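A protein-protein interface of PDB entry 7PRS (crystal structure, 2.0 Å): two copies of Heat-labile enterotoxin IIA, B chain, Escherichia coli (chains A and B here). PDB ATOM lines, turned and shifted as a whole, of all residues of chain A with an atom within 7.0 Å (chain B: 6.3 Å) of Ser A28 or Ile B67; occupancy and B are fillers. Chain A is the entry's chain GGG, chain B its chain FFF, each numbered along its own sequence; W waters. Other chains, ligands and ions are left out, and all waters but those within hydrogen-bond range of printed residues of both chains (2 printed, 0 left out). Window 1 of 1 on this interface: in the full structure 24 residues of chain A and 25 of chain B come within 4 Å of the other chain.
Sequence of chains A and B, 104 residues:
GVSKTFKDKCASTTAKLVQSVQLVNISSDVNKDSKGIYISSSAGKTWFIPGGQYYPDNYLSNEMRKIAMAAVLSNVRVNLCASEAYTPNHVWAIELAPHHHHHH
O of Leu B60 sits at hydrogen-bond distance from OG of Ser A28. O of Trp B92 sits at hydrogen-bond distance from N of Val A30 (2.9 Å). The backbone NH of Ile B94 is in hydrogen-bond range of the backbone carbonyl oxygen of Ser A28 (3.0 Å). N of Leu B96 lies within hydrogen-bond range of O of Ile A26 (2.8 Å).
The backbone carbonyl oxygen (O) of Ala B71 sits at hydrogen-bond distance from the backbone NH (N) of Val B76, at 3.0 Å. O of Tyr A38 lies within hydrogen-bond range of N of Ser A27. The side-chain carboxylate (OD1) of Asp A29 sits at hydrogen-bond distance from the backbone NH (N) of Asn A31 (2.8 Å). OG of Ser A34 is in hydrogen-bond range of OD2 of Asp A29, 2.6 Å away. The backbone carbonyl oxygen (O) of Asp A29 lies within hydrogen-bond range of the backbone NH (N) of Gly A36. The backbone carbonyl oxygen (O) of Val A30 lies within hydrogen-bond range of the side-chain amino group (NZ) of Lys A35 (3.1 Å).
Ile A26 touches Ile B67 (O to CD1, 3.8 Å). Ser A27 touches Ile B94 (CA to O, 3.0 Å). Met B64 touches Ser A28 (CG to OG, 3.7 Å). Ser A28 touches Ile B67 (N to CD1, 3.98 Å). Val A30 touches Leu B60 (CG1 to CB, 3.7 Å). Gly A36 touches Leu B60 (CA to CD2, 3.6 Å). CE1 of Tyr B59 touches CG1 of Ile A37, at 3.99 Å. Met A69 touches Glu B63. Leu A73 touches Ala B70 (CD2 to CB, 3.8 Å). Leu A73 touches Val B76 (CD1 to CG2, 3.9 Å).
Ser A28 touches just these residues of chain B: Leu B60 (2.8 Å), Glu B63 (3.9 Å), Met B64 (3.7 Å), Ile B67 (3.98 Å), Ala B93 (3.2 Å) and Ile B94 (3.0 Å). Lys A35 touches none of the printed residues of chain B. Printed residues of chain B within 4 Å of Leu A73: Ala B70 (3.8 Å) and Val B76 (3.9 Å). Of the printed residues of chain A, Tyr B59 touches Ile A37 (3.99 Å). Printed residues of chain A within 4 Å of Ile B67: Ile A26 (3.8 Å), Ser A28 (3.98 Å) and Met A69 (3.8 Å). Printed residues of chain A within 4 Å of Leu B96: Ile A26 (2.8 Å). The nearest residue of chain B that does not touch Ser A28 is Trp B92 (4.5 Å). The nearest printed residue of chain A that does not touch Glu B95 is Ser A28 (5.2 Å).
Of the 24 printed residues of chain B, 13 touch a printed residue of chain A. Printed residues of chain B that touch a printed residue of chain A: Phe B6, Tyr B59, Leu B60, Glu B63, Met B64, Ile B67, Ala B70, Val B76, Trp B92, Ala B93, Ile B94, Glu B95 and Leu B96. Hydrophobic or aromatic side chains of chain B within 4 Å of the printed part of chain A: Phe B6, Tyr B59, Leu B60, Met B64, Ile B67, Ala B70, Val B76, Trp B92, Ala B93 and Leu B96. Hydrophobic or aromatic side chains of chain A that line the printed part of chain B: Ile A26, Val A30, Ile A37, Met A69 and Leu A73. Among the printed residues, no Asp or Glu carboxylate lies within 4 Å of a Lys or Arg side-chain nitrogen of the other chain.
1 position is printed for both chains.
Water W2 lies within hydrogen-bond range of the side-chain carboxylate (OE2) of Glu B95 (2.7 Å), the side-chain hydroxyl (OG) of Ser A27 (2.9 Å) and the backbone carbonyl oxygen (O) of Tyr A38 (3.2 Å). Water W1 bridges OH of Tyr B59 (2.8 Å) and N of Ile A37 (2.9 Å).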
ATOM      1  N   ILE A  26      22.689  11.093 -29.296  1.00  0.00           N
ATOM      2  CA  ILE A  26      22.215  11.977 -28.201  1.00  0.00           C
ATOM      3  C   ILE A  26      21.437  13.082 -28.891  1.00  0.00           C
ATOM      4  O   ILE A  26      21.890  13.588 -29.938  1.00  0.00           O
ATOM      5  CB  ILE A  26      23.390  12.524 -27.341  1.00  0.00           C
ATOM      6  CG1 ILE A  26      22.848  13.463 -26.239  1.00  0.00           C
ATOM      7  CG2 ILE A  26      24.451  13.206 -28.180  1.00  0.00           C
ATOM      8  CD1 ILE A  26      23.909  13.858 -25.221  1.00  0.00           C
ATOM      9  N   SER A  27      20.329  13.471 -28.306  1.00  0.00           N
ATOM     10  CA  SER A  27      19.471  14.509 -28.918  1.00  0.00           C
ATOM     11  C   SER A  27      19.023  15.473 -27.840  1.00  0.00           C
ATOM     12  O   SER A  27      18.981  15.138 -26.664  1.00  0.00           O
ATOM     13  CB  SER A  27      18.263  13.871 -29.596  1.00  0.00           C
ATOM     14  OG  SER A  27      17.574  13.050 -28.671  1.00  0.00           O
ATOM     15  N   SER A  28      18.747  16.678 -28.273  1.00  0.00           N
ATOM     16  CA  SER A  28      18.097  17.701 -27.451  1.00  0.00           C
ATOM     17  C   SER A  28      16.847  18.126 -28.225  1.00  0.00           C
ATOM     18  O   SER A  28      16.972  18.394 -29.441  1.00  0.00           O
ATOM     19  CB  SER A  28      19.008  18.858 -27.213  1.00  0.00           C
ATOM     20  OG  SER A  28      18.385  19.817 -26.372  1.00  0.00           O
ATOM     21  N   ASP A  29      15.762  18.291 -27.500  1.00  0.00           N
ATOM     22  CA  ASP A  29      14.401  18.468 -28.062  1.00  0.00           C
ATOM     23  C   ASP A  29      13.761  19.595 -27.245  1.00  0.00           C
ATOM     24  O   ASP A  29      13.758  19.467 -26.008  1.00  0.00           O
ATOM     25  CB  ASP A  29      13.694  17.126 -27.956  1.00  0.00           C
ATOM     26  CG  ASP A  29      12.258  17.085 -28.529  1.00  0.00           C
ATOM     27  OD1 ASP A  29      11.705  18.167 -28.814  1.00  0.00           O
ATOM     28  OD2 ASP A  29      11.708  15.979 -28.622  1.00  0.00           O
ATOM     29  N   VAL A  30      13.355  20.689 -27.892  1.00  0.00           N
ATOM     30  CA  VAL A  30      12.594  21.773 -27.194  1.00  0.00           C
ATOM     31  C   VAL A  30      11.092  21.733 -27.580  1.00  0.00           C
ATOM     32  O   VAL A  30      10.378  22.664 -27.197  1.00  0.00           O
ATOM     33  CB  VAL A  30      13.223  23.147 -27.460  1.00  0.00           C
ATOM     34  CG1 VAL A  30      14.641  23.230 -26.905  1.00  0.00           C
ATOM     35  CG2 VAL A  30      13.207  23.487 -28.954  1.00  0.00           C
ATOM     36  N   ASN A  31      10.602  20.653 -28.170  1.00  0.00           N
ATOM     37  CA  ASN A  31       9.134  20.528 -28.480  1.00  0.00           C
ATOM     38  C   ASN A  31       8.309  20.435 -27.199  1.00  0.00           C
ATOM     39  O   ASN A  31       8.711  19.694 -26.274  1.00  0.00           O
ATOM     40  CB  ASN A  31       8.837  19.353 -29.413  1.00  0.00           C
ATOM     41  CG  ASN A  31       9.283  19.653 -30.833  1.00  0.00           C
ATOM     42  OD1 ASN A  31      10.100  18.903 -31.420  1.00  0.00           O
ATOM     43  ND2 ASN A  31       8.822  20.759 -31.399  1.00  0.00           N
ATOM     44  N   SER A  34       7.739  16.938 -25.639  1.00  0.00           N
ATOM     45  CA  SER A  34       8.849  15.948 -25.624  1.00  0.00           C
ATOM     46  C   SER A  34      10.180  16.587 -25.180  1.00  0.00           C
ATOM     47  O   SER A  34      11.173  15.916 -25.292  1.00  0.00           O
ATOM     48  CB  SER A  34       8.936  15.285 -26.991  1.00  0.00           C
ATOM     49  OG  SER A  34       9.163  16.267 -28.017  1.00  0.00           O
ATOM     50  N   LYS A  35      10.146  17.795 -24.620  1.00  0.00           N
ATOM     51  CA  LYS A  35      11.312  18.573 -24.117  1.00  0.00           C
ATOM     52  C   LYS A  35      12.279  17.628 -23.372  1.00  0.00           C
ATOM     53  O   LYS A  35      11.828  16.922 -22.482  1.00  0.00           O
ATOM     54  CB  LYS A  35      10.857  19.654 -23.145  1.00  0.00           C
ATOM     55  CG  LYS A  35      10.545  20.966 -23.825  1.00  0.00           C
ATOM     56  CD  LYS A  35      10.338  22.079 -22.828  1.00  0.00           C
ATOM     57  CE  LYS A  35       9.433  23.189 -23.318  1.00  0.00           C
ATOM     58  NZ  LYS A  35      10.076  23.997 -24.379  1.00  0.00           N
ATOM     59  N   GLY A  36      13.570  17.613 -23.730  1.00  0.00           N
ATOM     60  CA  GLY A  36      14.550  16.901 -22.907  1.00  0.00           C
ATOM     61  C   GLY A  36      15.729  16.388 -23.711  1.00  0.00           C
ATOM     62  O   GLY A  36      15.824  16.663 -24.968  1.00  0.00           O
ATOM     63  N   ILE A  37      16.617  15.692 -23.014  1.00  0.00           N
ATOM     64  CA  ILE A  37      17.831  15.062 -23.583  1.00  0.00           C
ATOM     65  C   ILE A  37      17.568  13.566 -23.633  1.00  0.00           C
ATOM     66  O   ILE A  37      17.192  12.984 -22.610  1.00  0.00           O
ATOM     67  CB  ILE A  37      19.044  15.407 -22.706  1.00  0.00           C
ATOM     68  CG1 ILE A  37      19.193  16.929 -22.563  1.00  0.00           C
ATOM     69  CG2 ILE A  37      20.291  14.684 -23.203  1.00  0.00           C
ATOM     70  CD1 ILE A  37      19.575  17.620 -23.835  1.00  0.00           C
ATOM     71  N   TYR A  38      17.789  12.976 -24.799  1.00  0.00           N
ATOM     72  CA  TYR A  38      17.656  11.532 -24.976  1.00  0.00           C
ATOM     73  C   TYR A  38      18.978  11.004 -25.481  1.00  0.00           C
ATOM     74  O   TYR A  38      19.630  11.690 -26.256  1.00  0.00           O
ATOM     75  CB  TYR A  38      16.492  11.178 -25.928  1.00  0.00           C
ATOM     76  CG  TYR A  38      15.172  11.764 -25.513  1.00  0.00           C
ATOM     77  CD1 TYR A  38      14.879  13.085 -25.793  1.00  0.00           C
ATOM     78  CD2 TYR A  38      14.213  11.018 -24.850  1.00  0.00           C
ATOM     79  CE1 TYR A  38      13.655  13.651 -25.451  1.00  0.00           C
ATOM     80  CE2 TYR A  38      12.999  11.582 -24.477  1.00  0.00           C
ATOM     81  CZ  TYR A  38      12.717  12.903 -24.784  1.00  0.00           C
ATOM     82  OH  TYR A  38      11.528  13.493 -24.461  1.00  0.00           O
ATOM     83  N   MET A  69      27.488  12.984 -24.159  1.00  0.00           N
ATOM     84  CA  MET A  69      27.905  13.618 -25.428  1.00  0.00           C
ATOM     85  C   MET A  69      29.264  13.056 -25.868  1.00  0.00           C
ATOM     86  O   MET A  69      29.444  12.673 -27.060  1.00  0.00           O
ATOM     87  CB  MET A  69      27.969  15.113 -25.209  1.00  0.00           C
ATOM     88  CG  MET A  69      28.453  15.868 -26.389  1.00  0.00           C
ATOM     89  SD  MET A  69      27.105  16.311 -27.411  1.00  0.00           S
ATOM     90  CE  MET A  69      26.133  17.428 -26.384  1.00  0.00           C
ATOM     91  N   LEU A  73      30.172  11.008 -29.237  1.00  0.00           N
ATOM     92  CA  LEU A  73      31.046  11.653 -30.212  1.00  0.00           C
ATOM     93  C   LEU A  73      32.340  10.822 -30.291  1.00  0.00           C
ATOM     94  O   LEU A  73      32.868  10.692 -31.403  1.00  0.00           O
ATOM     95  CB  LEU A  73      31.246  13.107 -29.807  1.00  0.00           C
ATOM     96  CG  LEU A  73      32.078  13.963 -30.737  1.00  0.00           C
ATOM     97  CD1 LEU A  73      31.455  14.011 -32.144  1.00  0.00           C
ATOM     98  CD2 LEU A  73      32.283  15.405 -30.159  1.00  0.00           C
ATOM     99  N   PHE B   6      13.473   9.636 -31.644  1.00  0.00           N
ATOM    100  CA  PHE B   6      13.670  10.940 -32.323  1.00  0.00           C
ATOM    101  C   PHE B   6      12.636  11.066 -33.449  1.00  0.00           C
ATOM    102  O   PHE B   6      11.976  12.122 -33.598  1.00  0.00           O
ATOM    103  CB  PHE B   6      15.097  11.115 -32.873  1.00  0.00           C
ATOM    104  CG  PHE B   6      15.385  12.521 -33.347  1.00  0.00           C
ATOM    105  CD1 PHE B   6      15.794  13.497 -32.440  1.00  0.00           C
ATOM    106  CD2 PHE B   6      15.193  12.904 -34.661  1.00  0.00           C
ATOM    107  CE1 PHE B   6      16.038  14.804 -32.861  1.00  0.00           C
ATOM    108  CE2 PHE B   6      15.415  14.205 -35.081  1.00  0.00           C
ATOM    109  CZ  PHE B   6      15.877  15.147 -34.183  1.00  0.00           C
ATOM    110  N   LEU B  23      26.466  18.837 -41.503  1.00  0.00           N
ATOM    111  CA  LEU B  23      26.637  20.289 -41.299  1.00  0.00           C
ATOM    112  C   LEU B  23      28.078  20.681 -41.642  1.00  0.00           C
ATOM    113  O   LEU B  23      29.011  20.034 -41.153  1.00  0.00           O
ATOM    114  CB  LEU B  23      26.266  20.715 -39.867  1.00  0.00           C
ATOM    115  CG  LEU B  23      24.826  20.400 -39.443  1.00  0.00           C
ATOM    116  CD1 LEU B  23      24.555  20.692 -37.989  1.00  0.00           C
ATOM    117  CD2 LEU B  23      23.852  21.172 -40.287  1.00  0.00           C
ATOM    118  N   TYR B  59      19.092  25.395 -21.135  1.00  0.00           N
ATOM    119  CA  TYR B  59      20.101  24.308 -21.211  1.00  0.00           C
ATOM    120  C   TYR B  59      19.821  23.460 -22.433  1.00  0.00           C
ATOM    121  O   TYR B  59      20.801  22.970 -23.050  1.00  0.00           O
ATOM    122  CB  TYR B  59      20.190  23.515 -19.907  1.00  0.00           C
ATOM    123  CG  TYR B  59      19.197  22.383 -19.801  1.00  0.00           C
ATOM    124  CD1 TYR B  59      19.434  21.148 -20.370  1.00  0.00           C
ATOM    125  CD2 TYR B  59      18.038  22.559 -19.050  1.00  0.00           C
ATOM    126  CE1 TYR B  59      18.527  20.112 -20.246  1.00  0.00           C
ATOM    127  CE2 TYR B  59      17.124  21.527 -18.910  1.00  0.00           C
ATOM    128  CZ  TYR B  59      17.389  20.275 -19.473  1.00  0.00           C
ATOM    129  OH  TYR B  59      16.485  19.236 -19.317  1.00  0.00           O
ATOM    130  N   LEU B  60      18.582  23.272 -22.860  1.00  0.00           N
ATOM    131  CA  LEU B  60      18.282  22.407 -24.008  1.00  0.00           C
ATOM    132  C   LEU B  60      18.822  23.079 -25.271  1.00  0.00           C
ATOM    133  O   LEU B  60      19.424  22.386 -26.128  1.00  0.00           O
ATOM    134  CB  LEU B  60      16.765  22.173 -24.108  1.00  0.00           C
ATOM    135  CG  LEU B  60      16.178  21.305 -22.990  1.00  0.00           C
ATOM    136  CD1 LEU B  60      14.660  21.398 -23.095  1.00  0.00           C
ATOM    137  CD2 LEU B  60      16.628  19.864 -23.103  1.00  0.00           C
ATOM    138  N   SER B  61      18.635  24.390 -25.401  1.00  0.00           N
ATOM    139  CA  SER B  61      19.121  25.126 -26.590  1.00  0.00           C
ATOM    140  C   SER B  61      20.660  25.072 -26.582  1.00  0.00           C
ATOM    141  O   SER B  61      21.257  24.894 -27.649  1.00  0.00           O
ATOM    142  CB  SER B  61      18.580  26.531 -26.675  1.00  0.00           C
ATOM    143  OG  SER B  61      19.097  27.328 -25.625  1.00  0.00           O
ATOM    144  N   ASN B  62      21.276  25.179 -25.416  1.00  0.00           N
ATOM    145  CA  ASN B  62      22.741  25.094 -25.280  1.00  0.00           C
ATOM    146  C   ASN B  62      23.198  23.712 -25.793  1.00  0.00           C
ATOM    147  O   ASN B  62      24.232  23.672 -26.468  1.00  0.00           O
ATOM    148  CB  ASN B  62      23.189  25.352 -23.844  1.00  0.00           C
ATOM    149  CG  ASN B  62      24.652  25.724 -23.768  1.00  0.00           C
ATOM    150  OD1 ASN B  62      25.183  26.483 -24.603  1.00  0.00           O
ATOM    151  ND2 ASN B  62      25.352  25.095 -22.840  1.00  0.00           N
ATOM    152  N   GLU B  63      22.500  22.625 -25.462  1.00  0.00           N
ATOM    153  CA  GLU B  63      22.874  21.273 -25.923  1.00  0.00           C
ATOM    154  C   GLU B  63      22.669  21.164 -27.412  1.00  0.00           C
ATOM    155  O   GLU B  63      23.546  20.525 -28.077  1.00  0.00           O
ATOM    156  CB  GLU B  63      22.124  20.166 -25.204  1.00  0.00           C
ATOM    157  CG  GLU B  63      22.400  20.147 -23.758  1.00  0.00           C
ATOM    158  CD  GLU B  63      23.851  19.924 -23.306  1.00  0.00           C
ATOM    159  OE1 GLU B  63      24.599  19.297 -24.040  1.00  0.00           O
ATOM    160  OE2 GLU B  63      24.173  20.389 -22.201  1.00  0.00           O
ATOM    161  N   MET B  64      21.627  21.783 -27.963  1.00  0.00           N
ATOM    162  CA  MET B  64      21.440  21.776 -29.420  1.00  0.00           C
ATOM    163  C   MET B  64      22.643  22.413 -30.104  1.00  0.00           C
ATOM    164  O   MET B  64      23.130  21.823 -31.076  1.00  0.00           O
ATOM    165  CB  MET B  64      20.164  22.510 -29.858  1.00  0.00           C
ATOM    166  CG  MET B  64      18.927  21.828 -29.388  1.00  0.00           C
ATOM    167  SD  MET B  64      17.450  22.482 -30.306  1.00  0.00           S
ATOM    168  CE  MET B  64      17.249  23.981 -29.367  1.00  0.00           C
ATOM    169  N   ARG B  65      23.113  23.522 -29.564  1.00  0.00           N
ATOM    170  CA  ARG B  65      24.302  24.233 -30.108  1.00  0.00           C
ATOM    171  C   ARG B  65      25.555  23.352 -29.991  1.00  0.00           C
ATOM    172  O   ARG B  65      26.297  23.255 -30.986  1.00  0.00           O
ATOM    173  CB  ARG B  65      24.457  25.577 -29.422  1.00  0.00           C
ATOM    174  CG  ARG B  65      23.290  26.531 -29.693  1.00  0.00           C
ATOM    175  CD  ARG B  65      23.620  27.931 -29.145  1.00  0.00           C
ATOM    176  NE  ARG B  65      23.825  28.051 -27.751  1.00  0.00           N
ATOM    177  CZ  ARG B  65      22.867  28.338 -26.840  1.00  0.00           C
ATOM    178  NH1 ARG B  65      21.611  28.519 -27.214  1.00  0.00           N
ATOM    179  NH2 ARG B  65      23.173  28.470 -25.579  1.00  0.00           N
ATOM    180  N   LYS B  66      25.773  22.682 -28.851  1.00  0.00           N
ATOM    181  CA  LYS B  66      26.953  21.830 -28.681  1.00  0.00           C
ATOM    182  C   LYS B  66      26.909  20.695 -29.684  1.00  0.00           C
ATOM    183  O   LYS B  66      27.984  20.365 -30.200  1.00  0.00           O
ATOM    184  CB  LYS B  66      27.046  21.273 -27.256  1.00  0.00           C
ATOM    185  CG  LYS B  66      27.303  22.239 -26.139  1.00  0.00           C
ATOM    186  CD  LYS B  66      27.491  21.607 -24.821  1.00  0.00           C
ATOM    187  CE  LYS B  66      27.770  22.603 -23.718  1.00  0.00           C
ATOM    188  NZ  LYS B  66      28.293  22.053 -22.448  1.00  0.00           N
ATOM    189  N   ILE B  67      25.726  20.109 -29.914  1.00  0.00           N
ATOM    190  CA  ILE B  67      25.591  19.014 -30.897  1.00  0.00           C
ATOM    191  C   ILE B  67      25.961  19.564 -32.290  1.00  0.00           C
ATOM    192  O   ILE B  67      26.779  18.909 -33.013  1.00  0.00           O
ATOM    193  CB  ILE B  67      24.184  18.392 -30.843  1.00  0.00           C
ATOM    194  CG1 ILE B  67      23.994  17.555 -29.580  1.00  0.00           C
ATOM    195  CG2 ILE B  67      23.900  17.580 -32.088  1.00  0.00           C
ATOM    196  CD1 ILE B  67      22.557  17.239 -29.259  1.00  0.00           C
ATOM    197  N   ALA B  68      25.375  20.694 -32.681  1.00  0.00           N
ATOM    198  CA  ALA B  68      25.636  21.259 -34.019  1.00  0.00           C
ATOM    199  C   ALA B  68      27.121  21.629 -34.182  1.00  0.00           C
ATOM    200  O   ALA B  68      27.705  21.363 -35.266  1.00  0.00           O
ATOM    201  CB  ALA B  68      24.727  22.449 -34.253  1.00  0.00           C
ATOM    202  N   MET B  69      27.721  22.205 -33.140  1.00  0.00           N
ATOM    203  CA  MET B  69      29.118  22.665 -33.203  1.00  0.00           C
ATOM    204  C   MET B  69      30.030  21.442 -33.425  1.00  0.00           C
ATOM    205  O   MET B  69      30.957  21.485 -34.289  1.00  0.00           O
ATOM    206  CB  MET B  69      29.441  23.370 -31.896  1.00  0.00           C
ATOM    207  CG  MET B  69      30.874  23.776 -31.762  1.00  0.00           C
ATOM    208  SD  MET B  69      31.097  25.433 -32.443  1.00  0.00           S
ATOM    209  CE  MET B  69      30.071  26.468 -31.379  1.00  0.00           C
ATOM    210  N   ALA B  70      29.815  20.396 -32.641  1.00  0.00           N
ATOM    211  CA  ALA B  70      30.576  19.127 -32.742  1.00  0.00           C
ATOM    212  C   ALA B  70      30.364  18.513 -34.125  1.00  0.00           C
ATOM    213  O   ALA B  70      31.334  17.994 -34.709  1.00  0.00           O
ATOM    214  CB  ALA B  70      30.167  18.192 -31.633  1.00  0.00           C
ATOM    215  N   ALA B  71      29.152  18.528 -34.643  1.00  0.00           N
ATOM    216  CA  ALA B  71      28.861  17.990 -35.992  1.00  0.00           C
ATOM    217  C   ALA B  71      29.712  18.708 -37.061  1.00  0.00           C
ATOM    218  O   ALA B  71      30.277  18.029 -37.928  1.00  0.00           O
ATOM    219  CB  ALA B  71      27.388  18.078 -36.278  1.00  0.00           C
ATOM    220  N   VAL B  72      29.809  20.030 -36.971  1.00  0.00           N
ATOM    221  CA  VAL B  72      30.595  20.834 -37.920  1.00  0.00           C
ATOM    222  C   VAL B  72      32.070  20.534 -37.732  1.00  0.00           C
ATOM    223  O   VAL B  72      32.760  20.209 -38.714  1.00  0.00           O
ATOM    224  CB  VAL B  72      30.303  22.329 -37.834  1.00  0.00           C
ATOM    225  CG1 VAL B  72      31.266  23.097 -38.753  1.00  0.00           C
ATOM    226  CG2 VAL B  72      28.879  22.584 -38.225  1.00  0.00           C
ATOM    227  N   VAL B  76      30.634  15.053 -38.477  1.00  0.00           N
ATOM    228  CA  VAL B  76      29.755  13.877 -38.210  1.00  0.00           C
ATOM    229  C   VAL B  76      28.294  14.306 -38.420  1.00  0.00           C
ATOM    230  O   VAL B  76      27.993  15.518 -38.315  1.00  0.00           O
ATOM    231  CB  VAL B  76      29.989  13.289 -36.811  1.00  0.00           C
ATOM    232  CG1 VAL B  76      31.374  12.640 -36.751  1.00  0.00           C
ATOM    233  CG2 VAL B  76      29.806  14.299 -35.699  1.00  0.00           C
ATOM    234  N   VAL B  78      24.062  14.590 -38.254  1.00  0.00           N
ATOM    235  CA  VAL B  78      22.931  14.800 -37.316  1.00  0.00           C
ATOM    236  C   VAL B  78      21.619  14.445 -38.018  1.00  0.00           C
ATOM    237  O   VAL B  78      21.555  14.442 -39.281  1.00  0.00           O
ATOM    238  CB  VAL B  78      22.893  16.244 -36.807  1.00  0.00           C
ATOM    239  CG1 VAL B  78      24.226  16.595 -36.110  1.00  0.00           C
ATOM    240  CG2 VAL B  78      22.586  17.230 -37.930  1.00  0.00           C
ATOM    241  N   VAL B  91      15.112  24.851 -36.004  1.00  0.00           N
ATOM    242  CA  VAL B  91      15.388  23.505 -35.437  1.00  0.00           C
ATOM    243  C   VAL B  91      14.625  23.392 -34.116  1.00  0.00           C
ATOM    244  O   VAL B  91      14.870  24.208 -33.199  1.00  0.00           O
ATOM    245  CB  VAL B  91      16.898  23.288 -35.212  1.00  0.00           C
ATOM    246  CG1 VAL B  91      17.179  21.921 -34.612  1.00  0.00           C
ATOM    247  CG2 VAL B  91      17.681  23.468 -36.497  1.00  0.00           C
ATOM    248  N   TRP B  92      13.790  22.360 -33.994  1.00  0.00           N
ATOM    249  CA  TRP B  92      13.075  22.100 -32.723  1.00  0.00           C
ATOM    250  C   TRP B  92      13.661  20.870 -32.036  1.00  0.00           C
ATOM    251  O   TRP B  92      13.424  20.716 -30.816  1.00  0.00           O
ATOM    252  CB  TRP B  92      11.577  21.946 -32.994  1.00  0.00           C
ATOM    253  CG  TRP B  92      10.895  23.242 -33.318  1.00  0.00           C
ATOM    254  CD1 TRP B  92      11.378  24.512 -33.204  1.00  0.00           C
ATOM    255  CD2 TRP B  92       9.553  23.377 -33.811  1.00  0.00           C
ATOM    256  NE1 TRP B  92      10.429  25.432 -33.602  1.00  0.00           N
ATOM    257  CE2 TRP B  92       9.293  24.757 -33.949  1.00  0.00           C
ATOM    258  CE3 TRP B  92       8.558  22.453 -34.134  1.00  0.00           C
ATOM    259  CZ2 TRP B  92       8.063  25.244 -34.400  1.00  0.00           C
ATOM    260  CZ3 TRP B  92       7.328  22.923 -34.551  1.00  0.00           C
ATOM    261  CH2 TRP B  92       7.089  24.302 -34.683  1.00  0.00           C
ATOM    262  N   ALA B  93      14.448  20.074 -32.750  1.00  0.00           N
ATOM    263  CA  ALA B  93      15.195  18.989 -32.096  1.00  0.00           C
ATOM    264  C   ALA B  93      16.371  18.624 -32.969  1.00  0.00           C
ATOM    265  O   ALA B  93      16.303  18.787 -34.217  1.00  0.00           O
ATOM    266  CB  ALA B  93      14.308  17.821 -31.774  1.00  0.00           C
ATOM    267  N   ILE B  94      17.451  18.166 -32.363  1.00  0.00           N
ATOM    268  CA  ILE B  94      18.627  17.728 -33.149  1.00  0.00           C
ATOM    269  C   ILE B  94      19.201  16.513 -32.447  1.00  0.00           C
ATOM    270  O   ILE B  94      19.221  16.466 -31.207  1.00  0.00           O
ATOM    271  CB  ILE B  94      19.654  18.888 -33.292  1.00  0.00           C
ATOM    272  CG1 ILE B  94      20.823  18.493 -34.200  1.00  0.00           C
ATOM    273  CG2 ILE B  94      20.152  19.368 -31.955  1.00  0.00           C
ATOM    274  CD1 ILE B  94      21.711  19.684 -34.559  1.00  0.00           C
ATOM    275  N   GLU B  95      19.668  15.574 -33.239  1.00  0.00           N
ATOM    276  CA  GLU B  95      20.272  14.323 -32.743  1.00  0.00           C
ATOM    277  C   GLU B  95      21.661  14.140 -33.385  1.00  0.00           C
ATOM    278  O   GLU B  95      21.762  14.156 -34.606  1.00  0.00           O
ATOM    279  CB  GLU B  95      19.375  13.136 -33.129  1.00  0.00           C
ATOM    280  CG  GLU B  95      19.933  11.789 -32.668  1.00  0.00           C
ATOM    281  CD  GLU B  95      18.850  10.695 -32.808  1.00  0.00           C
ATOM    282  OE1 GLU B  95      18.472  10.410 -33.968  1.00  0.00           O
ATOM    283  OE2 GLU B  95      18.388  10.155 -31.766  1.00  0.00           O
ATOM    284  N   LEU B  96      22.676  13.964 -32.562  1.00  0.00           N
ATOM    285  CA  LEU B  96      24.030  13.633 -33.052  1.00  0.00           C
ATOM    286  C   LEU B  96      23.976  12.156 -33.524  1.00  0.00           C
ATOM    287  O   LEU B  96      23.457  11.305 -32.767  1.00  0.00           O
ATOM    288  CB  LEU B  96      25.029  13.852 -31.915  1.00  0.00           C
ATOM    289  CG  LEU B  96      26.517  13.800 -32.263  1.00  0.00           C
ATOM    290  CD1 LEU B  96      26.900  14.821 -33.313  1.00  0.00           C
ATOM    291  CD2 LEU B  96      27.369  14.045 -31.020  1.00  0.00           C
HETATM  292  O   HOH W   1      16.259  16.619 -20.255  1.00  0.00           O
HETATM  293  O   HOH W   2      18.814  10.490 -29.132  1.00  0.00           O
